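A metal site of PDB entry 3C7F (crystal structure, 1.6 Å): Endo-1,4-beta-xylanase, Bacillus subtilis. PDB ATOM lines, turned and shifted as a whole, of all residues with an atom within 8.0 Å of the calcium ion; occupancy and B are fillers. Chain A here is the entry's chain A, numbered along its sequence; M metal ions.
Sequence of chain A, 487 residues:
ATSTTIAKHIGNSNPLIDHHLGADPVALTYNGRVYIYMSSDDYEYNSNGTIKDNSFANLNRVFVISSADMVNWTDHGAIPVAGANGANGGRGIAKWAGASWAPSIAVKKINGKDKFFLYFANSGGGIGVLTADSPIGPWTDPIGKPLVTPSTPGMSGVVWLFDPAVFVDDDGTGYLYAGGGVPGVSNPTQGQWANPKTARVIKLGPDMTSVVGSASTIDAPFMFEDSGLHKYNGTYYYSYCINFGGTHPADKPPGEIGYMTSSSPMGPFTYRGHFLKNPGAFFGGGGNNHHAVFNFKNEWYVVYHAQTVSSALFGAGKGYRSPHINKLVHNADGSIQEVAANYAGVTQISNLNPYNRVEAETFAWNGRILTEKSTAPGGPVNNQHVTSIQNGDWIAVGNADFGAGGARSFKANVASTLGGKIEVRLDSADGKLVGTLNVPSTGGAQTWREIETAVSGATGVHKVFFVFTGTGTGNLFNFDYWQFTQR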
ATOM      1  N   THR A  74      -3.782   7.734  14.400  1.00  0.00           N
ATOM      2  CA  THR A  74      -3.912   6.359  14.868  1.00  0.00           C
ATOM      3  C   THR A  74      -3.927   5.471  13.652  1.00  0.00           C
ATOM      4  O   THR A  74      -4.725   5.686  12.738  1.00  0.00           O
ATOM      5  CB  THR A  74      -5.252   6.142  15.632  1.00  0.00           C
ATOM      6  OG1 THR A  74      -5.329   7.093  16.696  1.00  0.00           O
ATOM      7  CG2 THR A  74      -5.340   4.722  16.180  1.00  0.00           C
ATOM      8  N   ASP A  75      -3.047   4.476  13.646  1.00  0.00           N
ATOM      9  CA  ASP A  75      -3.018   3.526  12.540  1.00  0.00           C
ATOM     10  C   ASP A  75      -3.971   2.377  12.856  1.00  0.00           C
ATOM     11  O   ASP A  75      -3.781   1.643  13.843  1.00  0.00           O
ATOM     12  CB  ASP A  75      -1.608   3.019  12.293  1.00  0.00           C
ATOM     13  CG  ASP A  75      -1.429   2.453  10.888  1.00  0.00           C
ATOM     14  OD1 ASP A  75      -2.244   1.594  10.488  1.00  0.00           O
ATOM     15  OD2 ASP A  75      -0.487   2.891  10.184  1.00  0.00           O
ATOM     16  N   ARG A 357      -6.096   5.792  27.776  1.00  0.00           N
ATOM     17  CA  ARG A 357      -5.357   4.843  26.959  1.00  0.00           C
ATOM     18  C   ARG A 357      -5.135   5.471  25.594  1.00  0.00           C
ATOM     19  O   ARG A 357      -6.093   5.907  24.914  1.00  0.00           O
ATOM     20  CB  ARG A 357      -6.110   3.516  26.792  1.00  0.00           C
ATOM     21  CG  ARG A 357      -5.423   2.552  25.858  1.00  0.00           C
ATOM     22  CD  ARG A 357      -6.108   1.192  25.768  1.00  0.00           C
ATOM     23  NE  ARG A 357      -5.654   0.465  24.579  1.00  0.00           N
ATOM     24  CZ  ARG A 357      -5.599  -0.863  24.466  1.00  0.00           C
ATOM     25  NH1 ARG A 357      -5.958  -1.636  25.476  1.00  0.00           N
ATOM     26  NH2 ARG A 357      -5.156  -1.407  23.340  1.00  0.00           N
ATOM     27  N   VAL A 358      -3.855   5.544  25.207  1.00  0.00           N
ATOM     28  CA  VAL A 358      -3.476   6.023  23.876  1.00  0.00           C
ATOM     29  C   VAL A 358      -2.741   4.859  23.203  1.00  0.00           C
ATOM     30  O   VAL A 358      -1.824   4.267  23.777  1.00  0.00           O
ATOM     31  CB  VAL A 358      -2.590   7.277  23.959  1.00  0.00           C
ATOM     32  CG1 VAL A 358      -2.196   7.743  22.567  1.00  0.00           C
ATOM     33  CG2 VAL A 358      -3.327   8.418  24.696  1.00  0.00           C
ATOM     34  N   GLU A 359      -3.199   4.469  22.020  1.00  0.00           N
ATOM     35  CA  GLU A 359      -2.500   3.396  21.307  1.00  0.00           C
ATOM     36  C   GLU A 359      -1.062   3.820  21.020  1.00  0.00           C
ATOM     37  O   GLU A 359      -0.812   4.994  20.704  1.00  0.00           O
ATOM     38  CB  GLU A 359      -3.220   3.074  19.995  1.00  0.00           C
ATOM     39  CG  GLU A 359      -4.637   2.556  20.182  1.00  0.00           C
ATOM     40  CD  GLU A 359      -4.735   1.448  21.207  1.00  0.00           C
ATOM     41  OE1 GLU A 359      -3.938   0.483  21.153  1.00  0.00           O
ATOM     42  OE2 GLU A 359      -5.619   1.546  22.072  1.00  0.00           O
ATOM     43  N   ALA A 360      -0.123   2.891  21.098  1.00  0.00           N
ATOM     44  CA  ALA A 360       1.245   3.224  20.708  1.00  0.00           C
ATOM     45  C   ALA A 360       1.306   3.615  19.223  1.00  0.00           C
ATOM     46  O   ALA A 360       2.107   4.454  18.819  1.00  0.00           O
ATOM     47  CB  ALA A 360       2.196   2.071  21.012  1.00  0.00           C
ATOM     48  N   GLU A 361       0.412   2.994  18.433  1.00  0.00           N
ATOM     49  CA  GLU A 361       0.275   3.306  17.003  1.00  0.00           C
ATOM     50  C   GLU A 361      -0.476   4.614  16.737  1.00  0.00           C
ATOM     51  O   GLU A 361      -0.853   4.899  15.581  1.00  0.00           O
ATOM     52  CB  GLU A 361      -0.387   2.130  16.276  1.00  0.00           C
ATOM     53  CG  GLU A 361      -1.839   1.903  16.644  1.00  0.00           C
ATOM     54  CD  GLU A 361      -2.034   0.893  17.788  1.00  0.00           C
ATOM     55  OE1 GLU A 361      -1.110   0.731  18.615  1.00  0.00           O
ATOM     56  OE2 GLU A 361      -3.127   0.269  17.878  1.00  0.00           O
ATOM     57  N   THR A 362      -0.704   5.419  17.785  1.00  0.00           N
ATOM     58  CA  THR A 362      -1.168   6.785  17.625  1.00  0.00           C
ATOM     59  C   THR A 362       0.018   7.708  17.838  1.00  0.00           C
ATOM     60  O   THR A 362       0.462   7.897  18.974  1.00  0.00           O
ATOM     61  CB  THR A 362      -2.258   7.145  18.651  1.00  0.00           C
ATOM     62  OG1 THR A 362      -3.402   6.315  18.408  1.00  0.00           O
ATOM     63  CG2 THR A 362      -2.650   8.641  18.539  1.00  0.00           C
ATOM     64  N   GLU A 372       1.716  -2.959  12.760  1.00  0.00           N
ATOM     65  CA  GLU A 372       1.092  -4.181  12.264  1.00  0.00           C
ATOM     66  C   GLU A 372       0.022  -4.643  13.251  1.00  0.00           C
ATOM     67  O   GLU A 372      -0.026  -4.168  14.394  1.00  0.00           O
ATOM     68  CB  GLU A 372       2.141  -5.287  12.074  1.00  0.00           C
ATOM     69  CG  GLU A 372       2.653  -5.850  13.377  1.00  0.00           C
ATOM     70  CD  GLU A 372       3.711  -6.943  13.225  1.00  0.00           C
ATOM     71  OE1 GLU A 372       4.069  -7.302  12.078  1.00  0.00           O
ATOM     72  OE2 GLU A 372       4.179  -7.429  14.282  1.00  0.00           O
ATOM     73  N   LYS A 373      -0.839  -5.550  12.797  1.00  0.00           N
ATOM     74  CA  LYS A 373      -1.892  -6.097  13.646  1.00  0.00           C
ATOM     75  C   LYS A 373      -1.258  -6.785  14.857  1.00  0.00           C
ATOM     76  O   LYS A 373      -0.273  -7.518  14.717  1.00  0.00           O
ATOM     77  CB  LYS A 373      -2.741  -7.090  12.846  1.00  0.00           C
ATOM     78  CG  LYS A 373      -4.073  -7.393  13.494  1.00  0.00           C
ATOM     79  CD  LYS A 373      -4.879  -8.370  12.639  1.00  0.00           C
ATOM     80  CE  LYS A 373      -6.283  -8.535  13.184  1.00  0.00           C
ATOM     81  NZ  LYS A 373      -6.295  -9.070  14.573  1.00  0.00           N
ATOM     82  N   SER A 374      -1.832  -6.544  16.027  1.00  0.00           N
ATOM     83  CA  SER A 374      -1.266  -7.030  17.287  1.00  0.00           C
ATOM     84  C   SER A 374      -1.928  -8.275  17.825  1.00  0.00           C
ATOM     85  O   SER A 374      -3.125  -8.485  17.639  1.00  0.00           O
ATOM     86  CB  SER A 374      -1.358  -5.931  18.353  1.00  0.00           C
ATOM     87  OG  SER A 374      -0.683  -6.331  19.532  1.00  0.00           O
ATOM     88  N   ALA A 376      -1.890  -8.585  21.087  1.00  0.00           N
ATOM     89  CA  ALA A 376      -2.214  -8.159  22.445  1.00  0.00           C
ATOM     90  C   ALA A 376      -3.681  -8.438  22.763  1.00  0.00           C
ATOM     91  O   ALA A 376      -4.548  -8.131  21.957  1.00  0.00           O
ATOM     92  CB  ALA A 376      -1.911  -6.692  22.635  1.00  0.00           C
ATOM     93  N   GLY A 378      -7.360  -7.845  24.137  1.00  0.00           N
ATOM     94  CA  GLY A 378      -8.207  -6.665  24.259  1.00  0.00           C
ATOM     95  C   GLY A 378      -7.880  -5.665  23.167  1.00  0.00           C
ATOM     96  O   GLY A 378      -7.421  -6.032  22.091  1.00  0.00           O
ATOM     97  N   GLY A 379      -8.113  -4.391  23.476  1.00  0.00           N
ATOM     98  CA  GLY A 379      -7.835  -3.322  22.555  1.00  0.00           C
ATOM     99  C   GLY A 379      -8.949  -3.098  21.540  1.00  0.00           C
ATOM    100  O   GLY A 379      -9.920  -3.870  21.474  1.00  0.00           O
ATOM    101  N   PRO A 380      -8.795  -2.040  20.729  1.00  0.00           N
ATOM    102  CA  PRO A 380      -9.830  -1.645  19.773  1.00  0.00           C
ATOM    103  C   PRO A 380      -9.919  -2.582  18.588  1.00  0.00           C
ATOM    104  O   PRO A 380      -9.100  -3.499  18.443  1.00  0.00           O
ATOM    105  CB  PRO A 380      -9.360  -0.265  19.314  1.00  0.00           C
ATOM    106  CG  PRO A 380      -7.864  -0.291  19.474  1.00  0.00           C
ATOM    107  CD  PRO A 380      -7.627  -1.134  20.704  1.00  0.00           C
ATOM    108  N   ASN A 382      -9.342  -4.191  15.216  1.00  0.00           N
ATOM    109  CA  ASN A 382      -8.125  -4.309  14.407  1.00  0.00           C
ATOM    110  C   ASN A 382      -6.906  -3.687  15.091  1.00  0.00           C
ATOM    111  O   ASN A 382      -6.027  -3.120  14.427  1.00  0.00           O
ATOM    112  CB  ASN A 382      -8.330  -3.714  13.005  1.00  0.00           C
ATOM    113  CG  ASN A 382      -7.539  -4.444  11.947  1.00  0.00           C
ATOM    114  OD1 ASN A 382      -7.445  -5.672  11.961  1.00  0.00           O
ATOM    115  ND2 ASN A 382      -6.962  -3.690  10.998  1.00  0.00           N
ATOM    116  N   ASN A 383      -6.870  -3.821  16.409  1.00  0.00           N
ATOM    117  CA  ASN A 383      -5.774  -3.278  17.206  1.00  0.00           C
ATOM    118  C   ASN A 383      -4.391  -3.576  16.614  1.00  0.00           C
ATOM    119  O   ASN A 383      -4.092  -4.725  16.217  1.00  0.00           O
ATOM    120  CB  ASN A 383      -5.872  -3.817  18.630  1.00  0.00           C
ATOM    121  CG  ASN A 383      -4.774  -3.280  19.542  1.00  0.00           C
ATOM    122  OD1 ASN A 383      -4.480  -2.081  19.536  1.00  0.00           O
ATOM    123  ND2 ASN A 383      -4.199  -4.166  20.343  1.00  0.00           N
ATOM    124  N   GLN A 384      -3.561  -2.539  16.536  1.00  0.00           N
ATOM    125  CA  GLN A 384      -2.211  -2.653  16.006  1.00  0.00           C
ATOM    126  C   GLN A 384      -1.196  -2.524  17.131  1.00  0.00           C
ATOM    127  O   GLN A 384      -1.549  -2.259  18.284  1.00  0.00           O
ATOM    128  CB  GLN A 384      -1.956  -1.550  14.960  1.00  0.00           C
ATOM    129  CG  GLN A 384      -3.007  -1.468  13.845  1.00  0.00           C
ATOM    130  CD  GLN A 384      -2.828  -2.538  12.784  1.00  0.00           C
ATOM    131  OE1 GLN A 384      -1.798  -2.573  12.108  1.00  0.00           O
ATOM    132  NE2 GLN A 384      -3.828  -3.397  12.629  1.00  0.00           N
ATOM    133  N   HIS A 385       0.067  -2.766  16.802  1.00  0.00           N
ATOM    134  CA  HIS A 385       1.150  -2.361  17.687  1.00  0.00           C
ATOM    135  C   HIS A 385       2.324  -1.782  16.917  1.00  0.00           C
ATOM    136  O   HIS A 385       2.394  -1.927  15.688  1.00  0.00           O
ATOM    137  CB  HIS A 385       1.585  -3.494  18.659  1.00  0.00           C
ATOM    138  CG  HIS A 385       2.050  -4.771  18.003  1.00  0.00           C
ATOM    139  ND1 HIS A 385       2.840  -4.800  16.871  1.00  0.00           N
ATOM    140  CD2 HIS A 385       1.878  -6.057  18.374  1.00  0.00           C
ATOM    141  CE1 HIS A 385       3.118  -6.059  16.572  1.00  0.00           C
ATOM    142  NE2 HIS A 385       2.537  -6.840  17.465  1.00  0.00           N
ATOM    143  N   VAL A 386       3.213  -1.097  17.634  1.00  0.00           N
ATOM    144  CA  VAL A 386       4.454  -0.619  17.046  1.00  0.00           C
ATOM    145  C   VAL A 386       5.492  -1.731  17.142  1.00  0.00           C
ATOM    146  O   VAL A 386       5.653  -2.357  18.206  1.00  0.00           O
ATOM    147  CB  VAL A 386       4.952   0.676  17.732  1.00  0.00           C
ATOM    148  CG1 VAL A 386       6.306   1.113  17.194  1.00  0.00           C
ATOM    149  CG2 VAL A 386       3.925   1.775  17.533  1.00  0.00           C
ATOM    150  N   ASN A 413       1.934  -1.191  27.565  1.00  0.00           N
ATOM    151  CA  ASN A 413       1.676  -2.602  27.290  1.00  0.00           C
ATOM    152  C   ASN A 413       2.684  -3.076  26.270  1.00  0.00           C
ATOM    153  O   ASN A 413       2.734  -2.554  25.155  1.00  0.00           O
ATOM    154  CB  ASN A 413       0.241  -2.803  26.767  1.00  0.00           C
ATOM    155  CG  ASN A 413      -0.252  -4.212  26.965  1.00  0.00           C
ATOM    156  OD1 ASN A 413       0.031  -4.843  27.986  1.00  0.00           O
ATOM    157  ND2 ASN A 413      -0.989  -4.742  25.973  1.00  0.00           N
ATOM    158  N   TRP A 448       2.080 -10.509  26.699  1.00  0.00           N
ATOM    159  CA  TRP A 448       1.934  -9.099  27.004  1.00  0.00           C
ATOM    160  C   TRP A 448       1.876  -8.774  28.488  1.00  0.00           C
ATOM    161  O   TRP A 448       1.207  -9.472  29.255  1.00  0.00           O
ATOM    162  CB  TRP A 448       0.695  -8.552  26.283  1.00  0.00           C
ATOM    163  CG  TRP A 448       0.877  -8.636  24.808  1.00  0.00           C
ATOM    164  CD1 TRP A 448       0.606  -9.711  24.017  1.00  0.00           C
ATOM    165  CD2 TRP A 448       1.423  -7.628  23.959  1.00  0.00           C
ATOM    166  NE1 TRP A 448       0.931  -9.424  22.707  1.00  0.00           N
ATOM    167  CE2 TRP A 448       1.436  -8.145  22.643  1.00  0.00           C
ATOM    168  CE3 TRP A 448       1.888  -6.314  24.170  1.00  0.00           C
ATOM    169  CZ2 TRP A 448       1.908  -7.408  21.543  1.00  0.00           C
ATOM    170  CZ3 TRP A 448       2.363  -5.583  23.082  1.00  0.00           C
ATOM    171  CH2 TRP A 448       2.362  -6.130  21.780  1.00  0.00           C
ATOM    172  N   PHE A 479       5.022  -2.854  21.121  1.00  0.00           N
ATOM    173  CA  PHE A 479       4.503  -1.788  21.981  1.00  0.00           C
ATOM    174  C   PHE A 479       3.067  -1.492  21.548  1.00  0.00           C
ATOM    175  O   PHE A 479       2.842  -0.998  20.441  1.00  0.00           O
ATOM    176  CB  PHE A 479       5.446  -0.592  21.812  1.00  0.00           C
ATOM    177  CG  PHE A 479       5.122   0.628  22.668  1.00  0.00           C
ATOM    178  CD1 PHE A 479       4.323   0.563  23.809  1.00  0.00           C
ATOM    179  CD2 PHE A 479       5.689   1.855  22.319  1.00  0.00           C
ATOM    180  CE1 PHE A 479       4.047   1.727  24.576  1.00  0.00           C
ATOM    181  CE2 PHE A 479       5.437   3.020  23.062  1.00  0.00           C
ATOM    182  CZ  PHE A 479       4.616   2.955  24.203  1.00  0.00           C
ATOM    183  N   ASP A 480       2.101  -1.807  22.405  1.00  0.00           N
ATOM    184  CA  ASP A 480       0.662  -1.817  22.056  1.00  0.00           C
ATOM    185  C   ASP A 480      -0.077  -0.516  22.411  1.00  0.00           C
ATOM    186  O   ASP A 480      -0.797   0.052  21.575  1.00  0.00           O
ATOM    187  CB  ASP A 480      -0.002  -3.019  22.744  1.00  0.00           C
ATOM    188  CG  ASP A 480      -1.509  -3.063  22.566  1.00  0.00           C
ATOM    189  OD1 ASP A 480      -2.042  -2.609  21.530  1.00  0.00           O
ATOM    190  OD2 ASP A 480      -2.168  -3.587  23.493  1.00  0.00           O
ATOM    191  N   TYR A 481       0.068  -0.071  23.660  1.00  0.00           N
ATOM    192  CA  TYR A 481      -0.587   1.145  24.126  1.00  0.00           C
ATOM    193  C   TYR A 481       0.159   1.679  25.320  1.00  0.00           C
ATOM    194  O   TYR A 481       0.986   0.975  25.895  1.00  0.00           O
ATOM    195  CB  TYR A 481      -2.066   0.908  24.472  1.00  0.00           C
ATOM    196  CG  TYR A 481      -2.316   0.132  25.755  1.00  0.00           C
ATOM    197  CD1 TYR A 481      -2.233   0.751  27.003  1.00  0.00           C
ATOM    198  CD2 TYR A 481      -2.657  -1.222  25.716  1.00  0.00           C
ATOM    199  CE1 TYR A 481      -2.464   0.047  28.194  1.00  0.00           C
ATOM    200  CE2 TYR A 481      -2.896  -1.933  26.898  1.00  0.00           C
ATOM    201  CZ  TYR A 481      -2.785  -1.291  28.123  1.00  0.00           C
ATOM    202  OH  TYR A 481      -3.012  -2.009  29.297  1.00  0.00           O
ATOM    203  N   TRP A 482      -0.120   2.927  25.638  1.00  0.00           N
ATOM    204  CA  TRP A 482       0.428   3.542  26.840  1.00  0.00           C
ATOM    205  C   TRP A 482      -0.629   4.413  27.508  1.00  0.00           C
ATOM    206  O   TRP A 482      -1.687   4.681  26.935  1.00  0.00           O
ATOM    207  CB  TRP A 482       1.692   4.341  26.523  1.00  0.00           C
ATOM    208  CG  TRP A 482       1.573   5.355  25.391  1.00  0.00           C
ATOM    209  CD1 TRP A 482       1.911   5.167  24.075  1.00  0.00           C
ATOM    210  CD2 TRP A 482       1.106   6.714  25.496  1.00  0.00           C
ATOM    211  NE1 TRP A 482       1.691   6.321  23.365  1.00  0.00           N
ATOM    212  CE2 TRP A 482       1.198   7.285  24.201  1.00  0.00           C
ATOM    213  CE3 TRP A 482       0.627   7.499  26.557  1.00  0.00           C
ATOM    214  CZ2 TRP A 482       0.823   8.608  23.946  1.00  0.00           C
ATOM    215  CZ3 TRP A 482       0.252   8.813  26.297  1.00  0.00           C
ATOM    216  CH2 TRP A 482       0.361   9.362  25.001  1.00  0.00           C
HETATM  217 CA    CA M   1      -2.459  -0.894  19.983  1.00  0.00          CA
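The side-chain carboxylate of Glu 359 is in salt-bridge range of the guanidinium group of Arg 357 (2.7 Å). The side-chain carboxylate of Asp 480 is in salt-bridge range of the guanidinium group of Arg 357 (3.7 Å). N of Ala 360 lies close to O of Asp 480, at 3.0 Å. N of Asp 480 sits at hydrogen-bond distance from O of Asn 413, 2.9 Å away. O of Asn 382 is in hydrogen-bond range of NE2 of Gln 384, at 2.9 Å. The backbone NH (N) of Lys 373 is in hydrogen-bond range of the side-chain amide oxygen (OE1) of Gln 384 (3.2 Å). The backbone carbonyl oxygen (O) of Asn 383 sits at hydrogen-bond distance from the backbone NH (N) of Ser 374. N of Asp 75 lies within hydrogen-bond range of O of Glu 361 (3.0 Å).
Five residues have an atom within 4 Å of the calcium ion: Glu 359, Glu 361, Asn 383, Gln 384 and Asp 480.
The calcium ion is bound by OE1 of Glu 359 (2.3 Å), OD1 of Asp 480 (2.3 Å), O of Gln 384 (2.4 Å), OD1 of Asn 383 (2.4 Å), O of Asp 480 (2.5 Å), OE2 of Glu 361 (2.5 Å) and OE1 of Glu 361 (2.5 Å). The calcium ion has seven donor atoms within binding distance.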
